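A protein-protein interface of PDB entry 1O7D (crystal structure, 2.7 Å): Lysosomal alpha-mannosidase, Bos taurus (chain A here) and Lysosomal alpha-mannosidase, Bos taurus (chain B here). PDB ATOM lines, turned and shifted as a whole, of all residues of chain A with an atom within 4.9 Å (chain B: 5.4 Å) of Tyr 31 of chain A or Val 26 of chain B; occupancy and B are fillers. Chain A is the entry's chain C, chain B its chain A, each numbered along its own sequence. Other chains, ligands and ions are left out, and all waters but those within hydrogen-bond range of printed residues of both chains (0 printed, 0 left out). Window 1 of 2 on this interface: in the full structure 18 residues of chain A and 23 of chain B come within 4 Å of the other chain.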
ATOM      1  N   VAL A  12      10.183  15.245  -4.543  1.00  0.00           N
ATOM      2  CA  VAL A  12       8.750  15.220  -4.776  1.00  0.00           C
ATOM      3  C   VAL A  12       8.459  15.314  -6.262  1.00  0.00           C
ATOM      4  O   VAL A  12       7.714  14.503  -6.817  1.00  0.00           O
ATOM      5  CB  VAL A  12       8.041  16.398  -4.072  1.00  0.00           C
ATOM      6  CG1 VAL A  12       6.554  16.373  -4.381  1.00  0.00           C
ATOM      7  CG2 VAL A  12       8.254  16.316  -2.574  1.00  0.00           C
ATOM      8  N   LEU A  13       9.053  16.299  -6.917  1.00  0.00           N
ATOM      9  CA  LEU A  13       8.800  16.466  -8.330  1.00  0.00           C
ATOM     10  C   LEU A  13       9.224  15.255  -9.150  1.00  0.00           C
ATOM     11  O   LEU A  13       8.890  15.135 -10.330  1.00  0.00           O
ATOM     12  CB  LEU A  13       9.495  17.722  -8.837  1.00  0.00           C
ATOM     13  CG  LEU A  13       9.006  19.045  -8.240  1.00  0.00           C
ATOM     14  CD1 LEU A  13       9.788  20.086  -8.916  1.00  0.00           C
ATOM     15  CD2 LEU A  13       7.545  19.325  -8.477  1.00  0.00           C
ATOM     16  N   HIS A  15       8.195  12.395  -8.624  1.00  0.00           N
ATOM     17  CA  HIS A  15       7.052  11.479  -8.636  1.00  0.00           C
ATOM     18  C   HIS A  15       6.669  11.161 -10.092  1.00  0.00           C
ATOM     19  O   HIS A  15       7.177  11.800 -11.018  1.00  0.00           O
ATOM     20  CB  HIS A  15       5.876  12.148  -7.931  1.00  0.00           C
ATOM     21  CG  HIS A  15       4.644  11.279  -7.872  1.00  0.00           C
ATOM     22  ND1 HIS A  15       4.597  10.108  -7.154  1.00  0.00           N
ATOM     23  CD2 HIS A  15       3.444  11.421  -8.471  1.00  0.00           C
ATOM     24  CE1 HIS A  15       3.398   9.556  -7.314  1.00  0.00           C
ATOM     25  NE2 HIS A  15       2.685  10.325  -8.102  1.00  0.00           N
ATOM     26  N   ASP A  17       3.558  11.456 -11.364  1.00  0.00           N
ATOM     27  CA  ASP A  17       2.448  12.277 -11.778  1.00  0.00           C
ATOM     28  C   ASP A  17       2.868  13.731 -11.735  1.00  0.00           C
ATOM     29  O   ASP A  17       2.076  14.606 -12.079  1.00  0.00           O
ATOM     30  CB  ASP A  17       1.253  12.117 -10.835  1.00  0.00           C
ATOM     31  CG  ASP A  17       0.664  10.743 -10.865  1.00  0.00           C
ATOM     32  OD1 ASP A  17       0.696  10.146 -11.962  1.00  0.00           O
ATOM     33  OD2 ASP A  17       0.159  10.275  -9.810  1.00  0.00           O
ATOM     34  N   ALA A  18       4.096  13.998 -11.297  1.00  0.00           N
ATOM     35  CA  ALA A  18       4.584  15.383 -11.203  1.00  0.00           C
ATOM     36  C   ALA A  18       5.274  15.945 -12.457  1.00  0.00           C
ATOM     37  O   ALA A  18       4.650  16.633 -13.251  1.00  0.00           O
ATOM     38  CB  ALA A  18       5.513  15.528  -9.972  1.00  0.00           C
ATOM     39  N   SER A  23      -0.625  15.396 -13.512  1.00  0.00           N
ATOM     40  CA  SER A  23      -1.435  15.667 -12.338  1.00  0.00           C
ATOM     41  C   SER A  23      -2.357  16.836 -12.649  1.00  0.00           C
ATOM     42  O   SER A  23      -2.201  17.513 -13.666  1.00  0.00           O
ATOM     43  CB  SER A  23      -0.543  16.002 -11.144  1.00  0.00           C
ATOM     44  OG  SER A  23       0.339  17.066 -11.463  1.00  0.00           O
ATOM     45  N   VAL A  27      -2.419  20.640  -8.327  1.00  0.00           N
ATOM     46  CA  VAL A  27      -1.283  19.866  -7.838  1.00  0.00           C
ATOM     47  C   VAL A  27      -0.043  20.317  -8.602  1.00  0.00           C
ATOM     48  O   VAL A  27       1.052  20.328  -8.067  1.00  0.00           O
ATOM     49  CB  VAL A  27      -1.530  18.352  -8.009  1.00  0.00           C
ATOM     50  CG1 VAL A  27      -0.289  17.554  -7.678  1.00  0.00           C
ATOM     51  CG2 VAL A  27      -2.659  17.936  -7.089  1.00  0.00           C
ATOM     52  N   ALA A  28      -0.227  20.706  -9.859  1.00  0.00           N
ATOM     53  CA  ALA A  28       0.879  21.219 -10.663  1.00  0.00           C
ATOM     54  C   ALA A  28       1.309  22.604 -10.131  1.00  0.00           C
ATOM     55  O   ALA A  28       2.458  23.005 -10.279  1.00  0.00           O
ATOM     56  CB  ALA A  28       0.455  21.331 -12.119  1.00  0.00           C
ATOM     57  N   ASN A  29       0.382  23.339  -9.522  1.00  0.00           N
ATOM     58  CA  ASN A  29       0.709  24.641  -8.971  1.00  0.00           C
ATOM     59  C   ASN A  29       1.443  24.449  -7.639  1.00  0.00           C
ATOM     60  O   ASN A  29       2.443  25.109  -7.376  1.00  0.00           O
ATOM     61  CB  ASN A  29      -0.557  25.492  -8.770  1.00  0.00           C
ATOM     62  CG  ASN A  29      -1.215  25.903 -10.086  1.00  0.00           C
ATOM     63  OD1 ASN A  29      -0.543  26.171 -11.078  1.00  0.00           O
ATOM     64  ND2 ASN A  29      -2.540  25.977 -10.086  1.00  0.00           N
ATOM     65  N   ASP A  30       0.957  23.538  -6.805  1.00  0.00           N
ATOM     66  CA  ASP A  30       1.584  23.288  -5.512  1.00  0.00           C
ATOM     67  C   ASP A  30       2.961  22.642  -5.680  1.00  0.00           C
ATOM     68  O   ASP A  30       3.796  22.726  -4.780  1.00  0.00           O
ATOM     69  CB  ASP A  30       0.677  22.397  -4.649  1.00  0.00           C
ATOM     70  CG  ASP A  30       1.321  21.990  -3.322  1.00  0.00           C
ATOM     71  OD1 ASP A  30       1.515  22.842  -2.437  1.00  0.00           O
ATOM     72  OD2 ASP A  30       1.629  20.800  -3.163  1.00  0.00           O
ATOM     73  N   TYR A  31       3.200  21.999  -6.822  1.00  0.00           N
ATOM     74  CA  TYR A  31       4.500  21.381  -7.056  1.00  0.00           C
ATOM     75  C   TYR A  31       5.511  22.497  -7.237  1.00  0.00           C
ATOM     76  O   TYR A  31       6.576  22.504  -6.603  1.00  0.00           O
ATOM     77  CB  TYR A  31       4.498  20.505  -8.309  1.00  0.00           C
ATOM     78  CG  TYR A  31       3.966  19.101  -8.111  1.00  0.00           C
ATOM     79  CD1 TYR A  31       4.276  18.368  -6.968  1.00  0.00           C
ATOM     80  CD2 TYR A  31       3.175  18.491  -9.090  1.00  0.00           C
ATOM     81  CE1 TYR A  31       3.811  17.059  -6.804  1.00  0.00           C
ATOM     82  CE2 TYR A  31       2.708  17.183  -8.939  1.00  0.00           C
ATOM     83  CZ  TYR A  31       3.028  16.471  -7.793  1.00  0.00           C
ATOM     84  OH  TYR A  31       2.574  15.181  -7.633  1.00  0.00           O
ATOM     85  N   ALA A  32       5.172  23.442  -8.111  1.00  0.00           N
ATOM     86  CA  ALA A  32       6.040  24.581  -8.386  1.00  0.00           C
ATOM     87  C   ALA A  32       6.222  25.397  -7.111  1.00  0.00           C
ATOM     88  O   ALA A  32       7.294  25.960  -6.873  1.00  0.00           O
ATOM     89  CB  ALA A  32       5.441  25.450  -9.483  1.00  0.00           C
ATOM     90  N   ARG A  33       5.171  25.451  -6.299  1.00  0.00           N
ATOM     91  CA  ARG A  33       5.209  26.173  -5.040  1.00  0.00           C
ATOM     92  C   ARG A  33       6.256  25.584  -4.093  1.00  0.00           C
ATOM     93  O   ARG A  33       7.031  26.328  -3.501  1.00  0.00           O
ATOM     94  CB  ARG A  33       3.831  26.145  -4.380  1.00  0.00           C
ATOM     95  N   GLN A  34       6.279  24.260  -3.944  1.00  0.00           N
ATOM     96  CA  GLN A  34       7.263  23.600  -3.071  1.00  0.00           C
ATOM     97  C   GLN A  34       8.682  23.898  -3.542  1.00  0.00           C
ATOM     98  O   GLN A  34       9.594  24.015  -2.726  1.00  0.00           O
ATOM     99  CB  GLN A  34       7.071  22.070  -3.036  1.00  0.00           C
ATOM    100  CG  GLN A  34       5.920  21.569  -2.170  1.00  0.00           C
ATOM    101  CD  GLN A  34       5.752  20.042  -2.234  1.00  0.00           C
ATOM    102  OE1 GLN A  34       6.606  19.281  -1.746  1.00  0.00           O
ATOM    103  NE2 GLN A  34       4.649  19.588  -2.846  1.00  0.00           N
ATOM    104  N   LEU A  35       8.863  24.000  -4.857  1.00  0.00           N
ATOM    105  CA  LEU A  35      10.166  24.304  -5.436  1.00  0.00           C
ATOM    106  C   LEU A  35      10.588  25.740  -5.190  1.00  0.00           C
ATOM    107  O   LEU A  35      11.745  26.012  -4.916  1.00  0.00           O
ATOM    108  CB  LEU A  35      10.146  24.099  -6.937  1.00  0.00           C
ATOM    109  CG  LEU A  35      10.382  22.711  -7.483  1.00  0.00           C
ATOM    110  CD1 LEU A  35      10.772  22.874  -8.940  1.00  0.00           C
ATOM    111  CD2 LEU A  35      11.481  22.005  -6.710  1.00  0.00           C
ATOM    112  N   ASP B  24       0.332   4.686  -3.013  1.00  0.00           N
ATOM    113  CA  ASP B  24       0.036   6.054  -2.582  1.00  0.00           C
ATOM    114  C   ASP B  24       0.767   7.091  -3.431  1.00  0.00           C
ATOM    115  O   ASP B  24       1.963   7.329  -3.261  1.00  0.00           O
ATOM    116  CB  ASP B  24       0.423   6.240  -1.116  1.00  0.00           C
ATOM    117  CG  ASP B  24      -0.335   5.309  -0.197  1.00  0.00           C
ATOM    118  OD1 ASP B  24      -1.260   4.626  -0.690  1.00  0.00           O
ATOM    119  OD2 ASP B  24      -0.011   5.268   1.015  1.00  0.00           O
ATOM    120  N   ASP B  25       0.040   7.721  -4.339  1.00  0.00           N
ATOM    121  CA  ASP B  25       0.646   8.705  -5.214  1.00  0.00           C
ATOM    122  C   ASP B  25       0.996   9.981  -4.464  1.00  0.00           C
ATOM    123  O   ASP B  25       0.137  10.600  -3.844  1.00  0.00           O
ATOM    124  CB  ASP B  25      -0.299   9.004  -6.385  1.00  0.00           C
ATOM    125  CG  ASP B  25      -0.456   7.818  -7.325  1.00  0.00           C
ATOM    126  OD1 ASP B  25       0.564   7.382  -7.883  1.00  0.00           O
ATOM    127  OD2 ASP B  25      -1.587   7.319  -7.511  1.00  0.00           O
ATOM    128  N   VAL B  26       2.268  10.358  -4.498  1.00  0.00           N
ATOM    129  CA  VAL B  26       2.697  11.586  -3.840  1.00  0.00           C
ATOM    130  C   VAL B  26       2.248  12.724  -4.763  1.00  0.00           C
ATOM    131  O   VAL B  26       3.050  13.372  -5.452  1.00  0.00           O
ATOM    132  CB  VAL B  26       4.239  11.608  -3.626  1.00  0.00           C
ATOM    133  CG1 VAL B  26       4.680  12.976  -3.123  1.00  0.00           C
ATOM    134  CG2 VAL B  26       4.642  10.524  -2.622  1.00  0.00           C
ATOM    135  N   GLY B  27       0.936  12.939  -4.770  1.00  0.00           N
ATOM    136  CA  GLY B  27       0.346  13.957  -5.605  1.00  0.00           C
ATOM    137  C   GLY B  27      -0.098  13.377  -6.939  1.00  0.00           C
ATOM    138  O   GLY B  27       0.596  12.549  -7.544  1.00  0.00           O
ATOM    139  N   TRP B  28      -1.282  13.793  -7.369  1.00  0.00           N
ATOM    140  CA  TRP B  28      -1.850  13.390  -8.648  1.00  0.00           C
ATOM    141  C   TRP B  28      -3.130  14.185  -8.890  1.00  0.00           C
ATOM    142  O   TRP B  28      -3.187  15.035  -9.789  1.00  0.00           O
ATOM    143  CB  TRP B  28      -2.158  11.891  -8.698  1.00  0.00           C
ATOM    144  CG  TRP B  28      -2.779  11.487  -9.989  1.00  0.00           C
ATOM    145  CD1 TRP B  28      -2.425  11.920 -11.231  1.00  0.00           C
ATOM    146  CD2 TRP B  28      -3.872  10.589 -10.176  1.00  0.00           C
ATOM    147  NE1 TRP B  28      -3.234  11.357 -12.183  1.00  0.00           N
ATOM    148  CE2 TRP B  28      -4.138  10.538 -11.561  1.00  0.00           C
ATOM    149  CE3 TRP B  28      -4.663   9.828  -9.309  1.00  0.00           C
ATOM    150  CZ2 TRP B  28      -5.153   9.750 -12.097  1.00  0.00           C
ATOM    151  CZ3 TRP B  28      -5.669   9.046  -9.843  1.00  0.00           C
ATOM    152  CH2 TRP B  28      -5.910   9.018 -11.223  1.00  0.00           C
ATOM    153  N   VAL B  32       0.091  16.713  -1.859  1.00  0.00           N
ATOM    154  CA  VAL B  32       0.729  15.835  -0.879  1.00  0.00           C
ATOM    155  C   VAL B  32       0.123  15.956   0.530  1.00  0.00           C
ATOM    156  O   VAL B  32      -0.093  14.953   1.213  1.00  0.00           O
ATOM    157  CB  VAL B  32       2.245  16.107  -0.812  1.00  0.00           C
ATOM    158  CG1 VAL B  32       2.904  15.131   0.125  1.00  0.00           C
ATOM    159  CG2 VAL B  32       2.843  15.994  -2.202  1.00  0.00           C
ATOM    160  N   TYR B  35      -3.378  14.472   0.558  1.00  0.00           N
ATOM    161  CA  TYR B  35      -3.327  13.020   0.523  1.00  0.00           C
ATOM    162  C   TYR B  35      -2.914  12.465   1.868  1.00  0.00           C
ATOM    163  O   TYR B  35      -3.457  11.462   2.312  1.00  0.00           O
ATOM    164  CB  TYR B  35      -2.333  12.509  -0.518  1.00  0.00           C
ATOM    165  CG  TYR B  35      -2.920  12.311  -1.893  1.00  0.00           C
ATOM    166  CD1 TYR B  35      -4.093  11.587  -2.069  1.00  0.00           C
ATOM    167  CD2 TYR B  35      -2.291  12.820  -3.021  1.00  0.00           C
ATOM    168  CE1 TYR B  35      -4.624  11.373  -3.335  1.00  0.00           C
ATOM    169  CE2 TYR B  35      -2.810  12.611  -4.291  1.00  0.00           C
ATOM    170  CZ  TYR B  35      -3.974  11.887  -4.443  1.00  0.00           C
ATOM    171  OH  TYR B  35      -4.467  11.659  -5.708  1.00  0.00           O
ATOM    172  N   GLU B  71       6.116   4.546  -0.478  1.00  0.00           N
ATOM    173  CA  GLU B  71       6.436   5.968  -0.539  1.00  0.00           C
ATOM    174  C   GLU B  71       7.003   6.530   0.768  1.00  0.00           C
ATOM    175  O   GLU B  71       6.270   6.812   1.721  1.00  0.00           O
ATOM    176  CB  GLU B  71       5.203   6.768  -0.984  1.00  0.00           C
ATOM    177  CG  GLU B  71       4.688   6.466  -2.407  1.00  0.00           C
ATOM    178  CD  GLU B  71       3.984   5.108  -2.524  1.00  0.00           C
ATOM    179  OE1 GLU B  71       3.365   4.682  -1.528  1.00  0.00           O
ATOM    180  OE2 GLU B  71       4.031   4.475  -3.609  1.00  0.00           O
ATOM    181  N   ALA B  73       8.182   9.446   1.402  1.00  0.00           N
ATOM    182  CA  ALA B  73       7.760  10.814   1.685  1.00  0.00           C
ATOM    183  C   ALA B  73       6.533  10.857   2.606  1.00  0.00           C
ATOM    184  O   ALA B  73       6.406  11.764   3.428  1.00  0.00           O
ATOM    185  CB  ALA B  73       7.472  11.552   0.393  1.00  0.00           C
ATOM    186  N   PHE B  74       5.629   9.888   2.467  1.00  0.00           N
ATOM    187  CA  PHE B  74       4.435   9.831   3.309  1.00  0.00           C
ATOM    188  C   PHE B  74       4.783   9.203   4.648  1.00  0.00           C
ATOM    189  O   PHE B  74       4.371   9.680   5.704  1.00  0.00           O
ATOM    190  CB  PHE B  74       3.326   9.003   2.644  1.00  0.00           C
ATOM    191  CG  PHE B  74       2.551   9.744   1.582  1.00  0.00           C
ATOM    192  CD1 PHE B  74       1.831  10.886   1.895  1.00  0.00           C
ATOM    193  CD2 PHE B  74       2.543   9.294   0.263  1.00  0.00           C
ATOM    194  CE1 PHE B  74       1.118  11.572   0.916  1.00  0.00           C
ATOM    195  CE2 PHE B  74       1.833   9.974  -0.723  1.00  0.00           C
ATOM    196  CZ  PHE B  74       1.121  11.117  -0.392  1.00  0.00           C
ATOM    197  N   TRP B 106      12.038   8.390  -2.070  1.00  0.00           N
ATOM    198  CA  TRP B 106      11.223   9.395  -1.410  1.00  0.00           C
ATOM    199  C   TRP B 106       9.853   9.258  -2.027  1.00  0.00           C
ATOM    200  O   TRP B 106       8.845   9.470  -1.362  1.00  0.00           O
ATOM    201  CB  TRP B 106      11.795  10.795  -1.656  1.00  0.00           C
ATOM    202  CG  TRP B 106      11.108  11.879  -0.891  1.00  0.00           C
ATOM    203  CD1 TRP B 106      10.331  12.851  -1.405  1.00  0.00           C
ATOM    204  CD2 TRP B 106      11.154  12.108   0.524  1.00  0.00           C
ATOM    205  NE1 TRP B 106       9.883  13.684  -0.412  1.00  0.00           N
ATOM    206  CE2 TRP B 106      10.375  13.250   0.785  1.00  0.00           C
ATOM    207  CE3 TRP B 106      11.777  11.457   1.597  1.00  0.00           C
ATOM    208  CZ2 TRP B 106      10.201  13.763   2.070  1.00  0.00           C
ATOM    209  CZ3 TRP B 106      11.600  11.970   2.880  1.00  0.00           C
ATOM    210  CH2 TRP B 106      10.816  13.112   3.101  1.00  0.00           C
ATOM    211  N   VAL B 107       9.848   8.884  -3.304  1.00  0.00           N
ATOM    212  CA  VAL B 107       8.638   8.663  -4.082  1.00  0.00           C
ATOM    213  C   VAL B 107       8.951   7.585  -5.107  1.00  0.00           C
ATOM    214  O   VAL B 107      10.082   7.121  -5.201  1.00  0.00           O
ATOM    215  CB  VAL B 107       8.219   9.915  -4.880  1.00  0.00           C
ATOM    216  CG1 VAL B 107       8.143  11.117  -3.975  1.00  0.00           C
ATOM    217  CG2 VAL B 107       9.191  10.157  -6.009  1.00  0.00           C
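Printed residues of chain B that touch a printed residue of chain A: Asp 25, Val 26, Gly 27, Trp 28, Trp 106 and Val 107. Hydrophobic or aromatic side chains of chain B within 4 Å of the printed part of chain A: Val 26, Trp 28, Trp 106 and Val 107. Along chain B the printed residues that touch a printed residue of chain A span positions 25 to 107. Of the 15 printed residues of chain A, 6 touch a printed residue of chain B. Among the printed residues, no Asp or Glu carboxylate lies within 4 Å of a Lys or Arg side-chain nitrogen of the other chain.
OH of Tyr 31 of chain A lies within hydrogen-bond range of O of Val 26 of chain B (2.9 Å). NE2 of His 15 of chain A lies within hydrogen-bond range of O of Gly 27 of chain B (3.1 Å). The backbone carbonyl oxygen (O) of Gly 27 of chain B sits close to the side-chain hydroxyl (OH) of Tyr 31 of chain A (3.3 Å). OD2 of Asp 17 of chain A sits close to OD1 of Asp 25 of chain B, 3.5 Å away. O of Gly 27 of chain B lies close to OD2 of Asp 17 of chain A (3.2 Å).
The backbone NH (N) of Ala 73 of chain B is in hydrogen-bond range of the backbone carbonyl oxygen (O) of Trp 106 of chain B (2.8 Å). NE2 of His 15 of chain A is in hydrogen-bond range of OD2 of Asp 17 of chain A (3.0 Å). OG of Ser 23 of chain A sits at hydrogen-bond distance from O of Asp 17 of chain A.
Printed residues of chain B within 4 Å of Val 12 of chain A: Trp 106. Of the printed residues of chain B, Val 27 of chain A touches Trp 28. Tyr 31 of chain A touches just these residues of chain B: Val 26 (2.9 Å) and Gly 27 (3.3 Å). Gln 34 of chain A touches none of the printed residues of chain B. Printed residues of chain A within 4 Å of Asp 25 of chain B: His 15 (3.6 Å) and Asp 17 (3.5 Å). Val 26 of chain B touches just these residues of chain A: His 15 (3.1 Å) and Tyr 31 (2.9 Å). The nearest printed residue of chain B that does not touch Val 12 of chain A is Val 26 of chain B (4.1 Å).
Among the printed residues, pairs that only touch across the chains: Val 12 of chain A with Trp 106 of chain B (3.8 Å), His 15 of chain A with Asp 25 of chain B (3.6 Å), His 15 of chain A with Val 26 of chain B (3.1 Å), His 15 of chain A with Val 107 of chain B (3.6 Å), Asp 17 of chain A with Trp 28 of chain B (3.0 Å), Ser 23 of chain A with Trp 28 of chain B (3.1 Å) and Val 27 of chain A with Trp 28 of chain B (3.9 Å).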
